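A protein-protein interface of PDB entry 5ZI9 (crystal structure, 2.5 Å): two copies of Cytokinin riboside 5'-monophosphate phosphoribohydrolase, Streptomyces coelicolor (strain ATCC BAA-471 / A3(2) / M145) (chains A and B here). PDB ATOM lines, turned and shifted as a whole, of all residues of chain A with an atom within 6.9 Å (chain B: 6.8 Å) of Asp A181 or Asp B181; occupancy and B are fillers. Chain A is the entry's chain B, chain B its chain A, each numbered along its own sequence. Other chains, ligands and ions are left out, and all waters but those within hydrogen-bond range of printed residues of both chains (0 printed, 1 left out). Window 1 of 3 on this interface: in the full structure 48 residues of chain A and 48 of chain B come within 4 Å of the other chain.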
ATOM      1  N   PHE A 156      -6.418  19.130  42.319  1.00  0.00           N
ATOM      2  CA  PHE A 156      -6.710  19.355  40.906  1.00  0.00           C
ATOM      3  C   PHE A 156      -6.102  18.340  39.939  1.00  0.00           C
ATOM      4  O   PHE A 156      -6.763  17.808  39.045  1.00  0.00           O
ATOM      5  CB  PHE A 156      -6.171  20.743  40.562  1.00  0.00           C
ATOM      6  CG  PHE A 156      -6.790  21.353  39.347  1.00  0.00           C
ATOM      7  CD1 PHE A 156      -8.135  21.837  39.371  1.00  0.00           C
ATOM      8  CD2 PHE A 156      -6.046  21.501  38.164  1.00  0.00           C
ATOM      9  CE1 PHE A 156      -8.718  22.430  38.240  1.00  0.00           C
ATOM     10  CE2 PHE A 156      -6.640  22.094  37.026  1.00  0.00           C
ATOM     11  CZ  PHE A 156      -7.963  22.555  37.071  1.00  0.00           C
ATOM     12  N   LYS A 160      -7.526  15.463  37.410  1.00  0.00           N
ATOM     13  CA  LYS A 160      -7.265  15.493  35.943  1.00  0.00           C
ATOM     14  C   LYS A 160      -6.940  14.147  35.347  1.00  0.00           C
ATOM     15  O   LYS A 160      -7.318  13.840  34.233  1.00  0.00           O
ATOM     16  CB  LYS A 160      -6.073  16.395  35.649  1.00  0.00           C
ATOM     17  CG  LYS A 160      -6.468  17.777  35.279  1.00  0.00           C
ATOM     18  CD  LYS A 160      -5.209  18.590  35.120  1.00  0.00           C
ATOM     19  CE  LYS A 160      -5.418  19.900  34.367  1.00  0.00           C
ATOM     20  NZ  LYS A 160      -6.828  20.279  34.053  1.00  0.00           N
ATOM     21  N   GLY A 176     -16.820  27.200  29.716  1.00  0.00           N
ATOM     22  CA  GLY A 176     -15.864  28.234  30.080  1.00  0.00           C
ATOM     23  C   GLY A 176     -14.423  27.760  30.117  1.00  0.00           C
ATOM     24  O   GLY A 176     -14.033  26.696  29.581  1.00  0.00           O
ATOM     25  N   LEU A 177     -13.623  28.566  30.781  1.00  0.00           N
ATOM     26  CA  LEU A 177     -12.196  28.300  30.959  1.00  0.00           C
ATOM     27  C   LEU A 177     -11.888  26.853  31.406  1.00  0.00           C
ATOM     28  O   LEU A 177     -10.978  26.193  30.863  1.00  0.00           O
ATOM     29  CB  LEU A 177     -11.643  29.281  31.995  1.00  0.00           C
ATOM     30  CG  LEU A 177     -11.811  30.759  31.627  1.00  0.00           C
ATOM     31  CD1 LEU A 177     -11.172  31.613  32.687  1.00  0.00           C
ATOM     32  CD2 LEU A 177     -11.209  31.073  30.276  1.00  0.00           C
ATOM     33  N   GLY A 178     -12.642  26.356  32.380  1.00  0.00           N
ATOM     34  CA  GLY A 178     -12.440  24.985  32.884  1.00  0.00           C
ATOM     35  C   GLY A 178     -12.606  23.896  31.854  1.00  0.00           C
ATOM     36  O   GLY A 178     -11.910  22.882  31.881  1.00  0.00           O
ATOM     37  N   THR A 179     -13.559  24.131  30.959  1.00  0.00           N
ATOM     38  CA  THR A 179     -13.905  23.202  29.922  1.00  0.00           C
ATOM     39  C   THR A 179     -12.822  23.225  28.852  1.00  0.00           C
ATOM     40  O   THR A 179     -12.438  22.192  28.396  1.00  0.00           O
ATOM     41  CB  THR A 179     -15.288  23.565  29.343  1.00  0.00           C
ATOM     42  OG1 THR A 179     -16.317  23.338  30.333  1.00  0.00           O
ATOM     43  CG2 THR A 179     -15.602  22.741  28.123  1.00  0.00           C
ATOM     44  N   LEU A 180     -12.338  24.399  28.474  1.00  0.00           N
ATOM     45  CA  LEU A 180     -11.241  24.518  27.510  1.00  0.00           C
ATOM     46  C   LEU A 180      -9.949  23.886  28.003  1.00  0.00           C
ATOM     47  O   LEU A 180      -9.200  23.320  27.217  1.00  0.00           O
ATOM     48  CB  LEU A 180     -10.942  25.975  27.204  1.00  0.00           C
ATOM     49  CG  LEU A 180     -12.092  26.752  26.592  1.00  0.00           C
ATOM     50  CD1 LEU A 180     -11.871  28.259  26.654  1.00  0.00           C
ATOM     51  CD2 LEU A 180     -12.254  26.308  25.157  1.00  0.00           C
ATOM     52  N   ASP A 181      -9.699  23.976  29.301  1.00  0.00           N
ATOM     53  CA  ASP A 181      -8.532  23.379  29.938  1.00  0.00           C
ATOM     54  C   ASP A 181      -8.467  21.868  29.699  1.00  0.00           C
ATOM     55  O   ASP A 181      -7.408  21.347  29.283  1.00  0.00           O
ATOM     56  CB  ASP A 181      -8.574  23.742  31.425  1.00  0.00           C
ATOM     57  CG  ASP A 181      -7.595  22.963  32.258  1.00  0.00           C
ATOM     58  OD1 ASP A 181      -6.493  22.646  31.782  1.00  0.00           O
ATOM     59  OD2 ASP A 181      -7.932  22.666  33.418  1.00  0.00           O
ATOM     60  N   GLU A 182      -9.599  21.189  29.930  1.00  0.00           N
ATOM     61  CA  GLU A 182      -9.763  19.751  29.614  1.00  0.00           C
ATOM     62  C   GLU A 182      -9.743  19.476  28.129  1.00  0.00           C
ATOM     63  O   GLU A 182      -9.083  18.563  27.674  1.00  0.00           O
ATOM     64  CB  GLU A 182     -11.043  19.194  30.214  1.00  0.00           C
ATOM     65  CG  GLU A 182     -11.005  19.155  31.747  1.00  0.00           C
ATOM     66  CD  GLU A 182      -9.853  18.320  32.387  1.00  0.00           C
ATOM     67  OE1 GLU A 182      -9.434  17.223  31.896  1.00  0.00           O
ATOM     68  OE2 GLU A 182      -9.353  18.793  33.444  1.00  0.00           O
ATOM     69  N   LEU A 183     -10.428  20.288  27.359  1.00  0.00           N
ATOM     70  CA  LEU A 183     -10.435  20.123  25.935  1.00  0.00           C
ATOM     71  C   LEU A 183      -9.027  20.056  25.388  1.00  0.00           C
ATOM     72  O   LEU A 183      -8.641  19.091  24.754  1.00  0.00           O
ATOM     73  CB  LEU A 183     -11.189  21.265  25.254  1.00  0.00           C
ATOM     74  CG  LEU A 183     -11.076  21.302  23.719  1.00  0.00           C
ATOM     75  CD1 LEU A 183     -11.570  19.998  23.122  1.00  0.00           C
ATOM     76  CD2 LEU A 183     -11.831  22.507  23.153  1.00  0.00           C
ATOM     77  N   PHE A 184      -8.262  21.096  25.643  1.00  0.00           N
ATOM     78  CA  PHE A 184      -6.917  21.162  25.095  1.00  0.00           C
ATOM     79  C   PHE A 184      -5.927  20.168  25.695  1.00  0.00           C
ATOM     80  O   PHE A 184      -4.956  19.839  25.069  1.00  0.00           O
ATOM     81  CB  PHE A 184      -6.424  22.587  25.073  1.00  0.00           C
ATOM     82  CG  PHE A 184      -7.064  23.411  23.968  1.00  0.00           C
ATOM     83  CD1 PHE A 184      -6.809  23.111  22.634  1.00  0.00           C
ATOM     84  CD2 PHE A 184      -7.943  24.441  24.250  1.00  0.00           C
ATOM     85  CE1 PHE A 184      -7.392  23.841  21.608  1.00  0.00           C
ATOM     86  CE2 PHE A 184      -8.541  25.167  23.236  1.00  0.00           C
ATOM     87  CZ  PHE A 184      -8.264  24.868  21.910  1.00  0.00           C
ATOM     88  N   GLU A 185      -6.230  19.627  26.857  1.00  0.00           N
ATOM     89  CA  GLU A 185      -5.446  18.574  27.472  1.00  0.00           C
ATOM     90  C   GLU A 185      -5.577  17.260  26.692  1.00  0.00           C
ATOM     91  O   GLU A 185      -4.589  16.580  26.425  1.00  0.00           O
ATOM     92  CB  GLU A 185      -5.993  18.383  28.875  1.00  0.00           C
ATOM     93  CG  GLU A 185      -5.186  17.593  29.871  1.00  0.00           C
ATOM     94  CD  GLU A 185      -5.746  17.829  31.277  1.00  0.00           C
ATOM     95  OE1 GLU A 185      -6.335  16.880  31.887  1.00  0.00           O
ATOM     96  OE2 GLU A 185      -5.656  19.006  31.710  1.00  0.00           O
ATOM     97  N   ALA A 186      -6.825  16.897  26.386  1.00  0.00           N
ATOM     98  CA  ALA A 186      -7.128  15.706  25.612  1.00  0.00           C
ATOM     99  C   ALA A 186      -6.565  15.805  24.205  1.00  0.00           C
ATOM    100  O   ALA A 186      -6.008  14.848  23.657  1.00  0.00           O
ATOM    101  CB  ALA A 186      -8.634  15.493  25.578  1.00  0.00           C
ATOM    102  N   THR A 188      -3.873  17.495  23.284  1.00  0.00           N
ATOM    103  CA  THR A 188      -2.416  17.359  23.154  1.00  0.00           C
ATOM    104  C   THR A 188      -2.007  15.939  23.500  1.00  0.00           C
ATOM    105  O   THR A 188      -1.079  15.383  22.902  1.00  0.00           O
ATOM    106  CB  THR A 188      -1.551  18.488  23.814  1.00  0.00           C
ATOM    107  OG1 THR A 188      -0.885  18.049  25.000  1.00  0.00           O
ATOM    108  CG2 THR A 188      -2.368  19.678  24.067  1.00  0.00           C
ATOM    109  N   LEU A 189      -2.763  15.324  24.387  1.00  0.00           N
ATOM    110  CA  LEU A 189      -2.548  13.951  24.720  1.00  0.00           C
ATOM    111  C   LEU A 189      -2.725  13.099  23.484  1.00  0.00           C
ATOM    112  O   LEU A 189      -1.964  12.163  23.275  1.00  0.00           O
ATOM    113  CB  LEU A 189      -3.485  13.506  25.845  1.00  0.00           C
ATOM    114  CG  LEU A 189      -3.049  13.872  27.274  1.00  0.00           C
ATOM    115  CD1 LEU A 189      -4.187  13.640  28.264  1.00  0.00           C
ATOM    116  CD2 LEU A 189      -1.837  13.063  27.700  1.00  0.00           C
ATOM    117  N   PHE B 156       1.629  12.660  32.540  1.00  0.00           N
ATOM    118  CA  PHE B 156       1.309  14.010  32.051  1.00  0.00           C
ATOM    119  C   PHE B 156       0.892  14.971  33.160  1.00  0.00           C
ATOM    120  O   PHE B 156       1.255  16.150  33.145  1.00  0.00           O
ATOM    121  CB  PHE B 156       0.217  13.949  30.945  1.00  0.00           C
ATOM    122  CG  PHE B 156      -1.217  13.882  31.456  1.00  0.00           C
ATOM    123  CD1 PHE B 156      -1.941  15.030  31.690  1.00  0.00           C
ATOM    124  CD2 PHE B 156      -1.842  12.688  31.658  1.00  0.00           C
ATOM    125  CE1 PHE B 156      -3.246  14.980  32.157  1.00  0.00           C
ATOM    126  CE2 PHE B 156      -3.146  12.642  32.107  1.00  0.00           C
ATOM    127  CZ  PHE B 156      -3.842  13.784  32.363  1.00  0.00           C
ATOM    128  N   LYS B 160       2.571  18.467  34.714  1.00  0.00           N
ATOM    129  CA  LYS B 160       1.743  19.688  34.648  1.00  0.00           C
ATOM    130  C   LYS B 160       1.780  20.442  35.930  1.00  0.00           C
ATOM    131  O   LYS B 160       1.834  21.678  35.965  1.00  0.00           O
ATOM    132  CB  LYS B 160       0.289  19.333  34.393  1.00  0.00           C
ATOM    133  CG  LYS B 160      -0.071  19.286  32.913  1.00  0.00           C
ATOM    134  CD  LYS B 160      -1.391  18.542  32.664  1.00  0.00           C
ATOM    135  CE  LYS B 160      -1.793  18.700  31.220  1.00  0.00           C
ATOM    136  NZ  LYS B 160      -2.068  20.126  30.923  1.00  0.00           N
ATOM    137  N   PHE B 170       3.208  32.549  34.394  1.00  0.00           N
ATOM    138  CA  PHE B 170       3.325  31.881  33.103  1.00  0.00           C
ATOM    139  C   PHE B 170       3.519  32.949  32.045  1.00  0.00           C
ATOM    140  O   PHE B 170       2.824  33.972  32.033  1.00  0.00           O
ATOM    141  CB  PHE B 170       2.018  31.123  32.748  1.00  0.00           C
ATOM    142  CG  PHE B 170       1.958  29.682  33.173  1.00  0.00           C
ATOM    143  CD1 PHE B 170       2.699  29.191  34.244  1.00  0.00           C
ATOM    144  CD2 PHE B 170       1.075  28.825  32.531  1.00  0.00           C
ATOM    145  CE1 PHE B 170       2.605  27.877  34.614  1.00  0.00           C
ATOM    146  CE2 PHE B 170       0.949  27.507  32.908  1.00  0.00           C
ATOM    147  CZ  PHE B 170       1.718  27.029  33.950  1.00  0.00           C
ATOM    148  N   GLY B 176       1.028  26.088  19.901  1.00  0.00           N
ATOM    149  CA  GLY B 176       0.028  25.132  19.463  1.00  0.00           C
ATOM    150  C   GLY B 176      -0.930  24.607  20.508  1.00  0.00           C
ATOM    151  O   GLY B 176      -1.258  25.285  21.468  1.00  0.00           O
ATOM    152  N   LEU B 177      -1.351  23.361  20.306  1.00  0.00           N
ATOM    153  CA  LEU B 177      -2.342  22.724  21.159  1.00  0.00           C
ATOM    154  C   LEU B 177      -1.840  22.601  22.597  1.00  0.00           C
ATOM    155  O   LEU B 177      -2.588  22.889  23.524  1.00  0.00           O
ATOM    156  CB  LEU B 177      -2.748  21.355  20.603  1.00  0.00           C
ATOM    157  CG  LEU B 177      -3.365  21.352  19.173  1.00  0.00           C
ATOM    158  CD1 LEU B 177      -3.759  19.930  18.760  1.00  0.00           C
ATOM    159  CD2 LEU B 177      -4.538  22.322  19.006  1.00  0.00           C
ATOM    160  N   GLY B 178      -0.585  22.168  22.769  1.00  0.00           N
ATOM    161  CA  GLY B 178       0.038  22.000  24.086  1.00  0.00           C
ATOM    162  C   GLY B 178       0.232  23.291  24.824  1.00  0.00           C
ATOM    163  O   GLY B 178       0.241  23.305  26.050  1.00  0.00           O
ATOM    164  N   THR B 179       0.405  24.369  24.071  1.00  0.00           N
ATOM    165  CA  THR B 179       0.515  25.689  24.618  1.00  0.00           C
ATOM    166  C   THR B 179      -0.850  26.151  25.098  1.00  0.00           C
ATOM    167  O   THR B 179      -0.978  26.669  26.194  1.00  0.00           O
ATOM    168  CB  THR B 179       1.136  26.625  23.583  1.00  0.00           C
ATOM    169  OG1 THR B 179       2.445  26.141  23.284  1.00  0.00           O
ATOM    170  CG2 THR B 179       1.280  28.047  24.087  1.00  0.00           C
ATOM    171  N   LEU B 180      -1.879  25.926  24.308  1.00  0.00           N
ATOM    172  CA  LEU B 180      -3.260  26.255  24.741  1.00  0.00           C
ATOM    173  C   LEU B 180      -3.718  25.499  25.984  1.00  0.00           C
ATOM    174  O   LEU B 180      -4.411  26.043  26.846  1.00  0.00           O
ATOM    175  CB  LEU B 180      -4.254  26.030  23.608  1.00  0.00           C
ATOM    176  CG  LEU B 180      -4.043  27.023  22.444  1.00  0.00           C
ATOM    177  CD1 LEU B 180      -4.575  26.481  21.120  1.00  0.00           C
ATOM    178  CD2 LEU B 180      -4.622  28.398  22.706  1.00  0.00           C
ATOM    179  N   ASP B 181      -3.301  24.249  26.065  1.00  0.00           N
ATOM    180  CA  ASP B 181      -3.507  23.411  27.210  1.00  0.00           C
ATOM    181  C   ASP B 181      -3.049  24.064  28.536  1.00  0.00           C
ATOM    182  O   ASP B 181      -3.844  24.238  29.465  1.00  0.00           O
ATOM    183  CB  ASP B 181      -2.773  22.103  26.959  1.00  0.00           C
ATOM    184  CG  ASP B 181      -2.955  21.097  28.065  1.00  0.00           C
ATOM    185  OD1 ASP B 181      -3.874  21.237  28.952  1.00  0.00           O
ATOM    186  OD2 ASP B 181      -2.141  20.118  28.035  1.00  0.00           O
ATOM    187  N   GLU B 182      -1.785  24.444  28.598  1.00  0.00           N
ATOM    188  CA  GLU B 182      -1.223  25.052  29.796  1.00  0.00           C
ATOM    189  C   GLU B 182      -1.793  26.417  30.042  1.00  0.00           C
ATOM    190  O   GLU B 182      -2.072  26.766  31.166  1.00  0.00           O
ATOM    191  CB  GLU B 182       0.311  25.142  29.684  1.00  0.00           C
ATOM    192  CG  GLU B 182       0.981  23.766  29.638  1.00  0.00           C
ATOM    193  CD  GLU B 182       0.886  23.012  30.957  1.00  0.00           C
ATOM    194  OE1 GLU B 182       0.609  23.677  31.999  1.00  0.00           O
ATOM    195  OE2 GLU B 182       1.089  21.756  30.936  1.00  0.00           O
ATOM    196  N   LEU B 183      -1.973  27.196  28.989  1.00  0.00           N
ATOM    197  CA  LEU B 183      -2.666  28.484  29.098  1.00  0.00           C
ATOM    198  C   LEU B 183      -4.032  28.391  29.822  1.00  0.00           C
ATOM    199  O   LEU B 183      -4.289  29.124  30.778  1.00  0.00           O
ATOM    200  CB  LEU B 183      -2.852  29.104  27.696  1.00  0.00           C
ATOM    201  CG  LEU B 183      -3.841  30.277  27.511  1.00  0.00           C
ATOM    202  CD1 LEU B 183      -3.594  31.419  28.487  1.00  0.00           C
ATOM    203  CD2 LEU B 183      -3.773  30.787  26.074  1.00  0.00           C
ATOM    204  N   PHE B 184      -4.903  27.501  29.362  1.00  0.00           N
ATOM    205  CA  PHE B 184      -6.228  27.408  29.970  1.00  0.00           C
ATOM    206  C   PHE B 184      -6.261  26.754  31.343  1.00  0.00           C
ATOM    207  O   PHE B 184      -7.165  27.022  32.092  1.00  0.00           O
ATOM    208  CB  PHE B 184      -7.233  26.758  29.002  1.00  0.00           C
ATOM    209  CG  PHE B 184      -7.656  27.687  27.927  1.00  0.00           C
ATOM    210  CD1 PHE B 184      -8.317  28.853  28.256  1.00  0.00           C
ATOM    211  CD2 PHE B 184      -7.375  27.430  26.598  1.00  0.00           C
ATOM    212  CE1 PHE B 184      -8.698  29.768  27.287  1.00  0.00           C
ATOM    213  CE2 PHE B 184      -7.759  28.337  25.617  1.00  0.00           C
ATOM    214  CZ  PHE B 184      -8.416  29.518  25.969  1.00  0.00           C
ATOM    215  N   GLU B 185      -5.280  25.911  31.643  1.00  0.00           N
ATOM    216  CA  GLU B 185      -5.140  25.273  32.934  1.00  0.00           C
ATOM    217  C   GLU B 185      -4.820  26.342  33.948  1.00  0.00           C
ATOM    218  O   GLU B 185      -5.445  26.414  34.967  1.00  0.00           O
ATOM    219  CB  GLU B 185      -3.986  24.290  32.859  1.00  0.00           C
ATOM    220  CG  GLU B 185      -3.823  23.352  34.018  1.00  0.00           C
ATOM    221  CD  GLU B 185      -2.770  22.280  33.709  1.00  0.00           C
ATOM    222  OE1 GLU B 185      -3.027  21.402  32.841  1.00  0.00           O
ATOM    223  OE2 GLU B 185      -1.669  22.331  34.307  1.00  0.00           O
ATOM    224  N   ALA B 186      -3.857  27.194  33.644  1.00  0.00           N
ATOM    225  CA  ALA B 186      -3.490  28.310  34.498  1.00  0.00           C
ATOM    226  C   ALA B 186      -4.644  29.257  34.725  1.00  0.00           C
ATOM    227  O   ALA B 186      -4.815  29.813  35.789  1.00  0.00           O
ATOM    228  CB  ALA B 186      -2.320  29.103  33.892  1.00  0.00           C
ATOM    229  N   THR B 188      -7.790  28.493  34.752  1.00  0.00           N
ATOM    230  CA  THR B 188      -8.862  27.981  35.619  1.00  0.00           C
ATOM    231  C   THR B 188      -8.336  27.830  37.025  1.00  0.00           C
ATOM    232  O   THR B 188      -9.121  27.894  37.968  1.00  0.00           O
ATOM    233  CB  THR B 188      -9.635  26.719  35.127  1.00  0.00           C
ATOM    234  OG1 THR B 188      -9.168  25.542  35.793  1.00  0.00           O
ATOM    235  CG2 THR B 188      -9.472  26.545  33.689  1.00  0.00           C
ATOM    236  N   LEU B 189      -7.021  27.691  37.160  1.00  0.00           N
ATOM    237  CA  LEU B 189      -6.398  27.632  38.469  1.00  0.00           C
ATOM    238  C   LEU B 189      -6.533  28.963  39.185  1.00  0.00           C
ATOM    239  O   LEU B 189      -6.816  29.002  40.367  1.00  0.00           O
ATOM    240  CB  LEU B 189      -4.918  27.213  38.357  1.00  0.00           C
ATOM    241  CG  LEU B 189      -4.650  25.722  38.022  1.00  0.00           C
ATOM    242  CD1 LEU B 189      -3.173  25.478  37.729  1.00  0.00           C
ATOM    243  CD2 LEU B 189      -5.104  24.760  39.118  1.00  0.00           C
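Of the 16 printed residues of chain B, 10 touch a printed residue of chain A. Hydrophobic or aromatic side chains of chain B within 4 Å of the printed part of chain A: Phe B156, Leu B177, Leu B180, Phe B184 and Leu B189. Among the printed residues, Asp or Glu carboxylates within 4 Å of a Lys or Arg side-chain nitrogen of the other chain: Glu A185 with Lys B160 (3.8 Å).
OE2 of Glu A185 lies within salt-bridge range of NZ of Lys B160, 3.8 Å away. The backbone NH (N) of Glu B185 sits close to the side-chain carboxylate (OD1) of Asp A181 (3.5 Å).
Lys A160 touches Phe B156, but with the chains exchanged Phe A156 does not touch Lys B160 (7.7 Å). Leu A177 touches Thr B188, and with the chains exchanged Thr A188 touches Leu B177. Asp A181 touches Thr B188, and with the chains exchanged Thr A188 touches Asp B181. Glu A185 touches Phe B156, but with the chains exchanged Phe A156 does not touch Glu B185 (4.3 Å). Positions printed for both chains: 156, 160, 176, 177, 178, 179, 180, 181, 182, 183, 184, 185, 186, 188 and 189. Of the 22 pairs that touch across the chains among the printed residues, 19 have their exchanged pair printed and touching as well.
Of chain B, only Asp B181 (3.6 Å), Phe B184 (3.6 Å), Glu B185 (3.2 Å) and Thr B188 (3.7 Å) come within 4 Å of Asp A181. Of chain A, only Asp A181 (3.6 Å), Phe A184 (3.7 Å), Glu A185 (3.4 Å) and Thr A188 (3.8 Å) come within 4 Å of Asp B181. Printed residues of chain B within 4 Å of Glu A185: Phe B156 (3.6 Å), Lys B160 (3.8 Å), Asp B181 (3.4 Å) and Glu B185 (3.7 Å). Of the printed residues of chain B, Lys A160 touches Phe B156 and Glu B185. Of the printed residues of chain A, Thr B188 touches Phe A156 (3.5 Å), Leu A177 (3.2 Å), Gly A178 (3.4 Å) and Asp A181 (3.7 Å). Glu A182 touches none of the printed residues of chain B. The nearest printed residue of chain A that does not touch Phe B156 is Glu A182 (6.6 Å).
NZ of Lys B160 is in salt-bridge range of OD2 of Asp B181 (2.9 Å). NZ of Lys B160 lies within salt-bridge range of OE2 of Glu B182. OE1 of Glu B185 lies within salt-bridge range of NZ of Lys B160, 2.5 Å away. The side-chain carboxylate (OD2) of Asp A181 is in salt-bridge range of the side-chain amino group (NZ) of Lys A160 (2.7 Å). The side-chain carboxylate (OE2) of Glu A182 is in salt-bridge range of the side-chain amino group (NZ) of Lys A160 (3.0 Å). NZ of Lys A160 is in salt-bridge range of OE2 of Glu A185 (2.9 Å).
Among the printed residues, merely in contact across the chains: Lys A160 with Glu B185, Leu A177 with Thr B188, Thr A188 with Leu B177, Thr A188 with Gly B178, Glu A185 with Asp B181, Gly A178 with Thr B188, Phe A156 with Thr B188, Phe A156 with Leu B189, Asp A181 with Asp B181, Leu A180 with Phe B184, Asp A181 with Phe B184, Glu A185 with Phe B156, Phe A184 with Asp B181, Asp A181 with Thr B188, Glu A185 with Glu B185, Thr A188 with Asp B181, Phe A184 with Phe B184, Phe A184 with Leu B180, Leu A189 with Phe B156 and Lys A160 with Phe B156.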
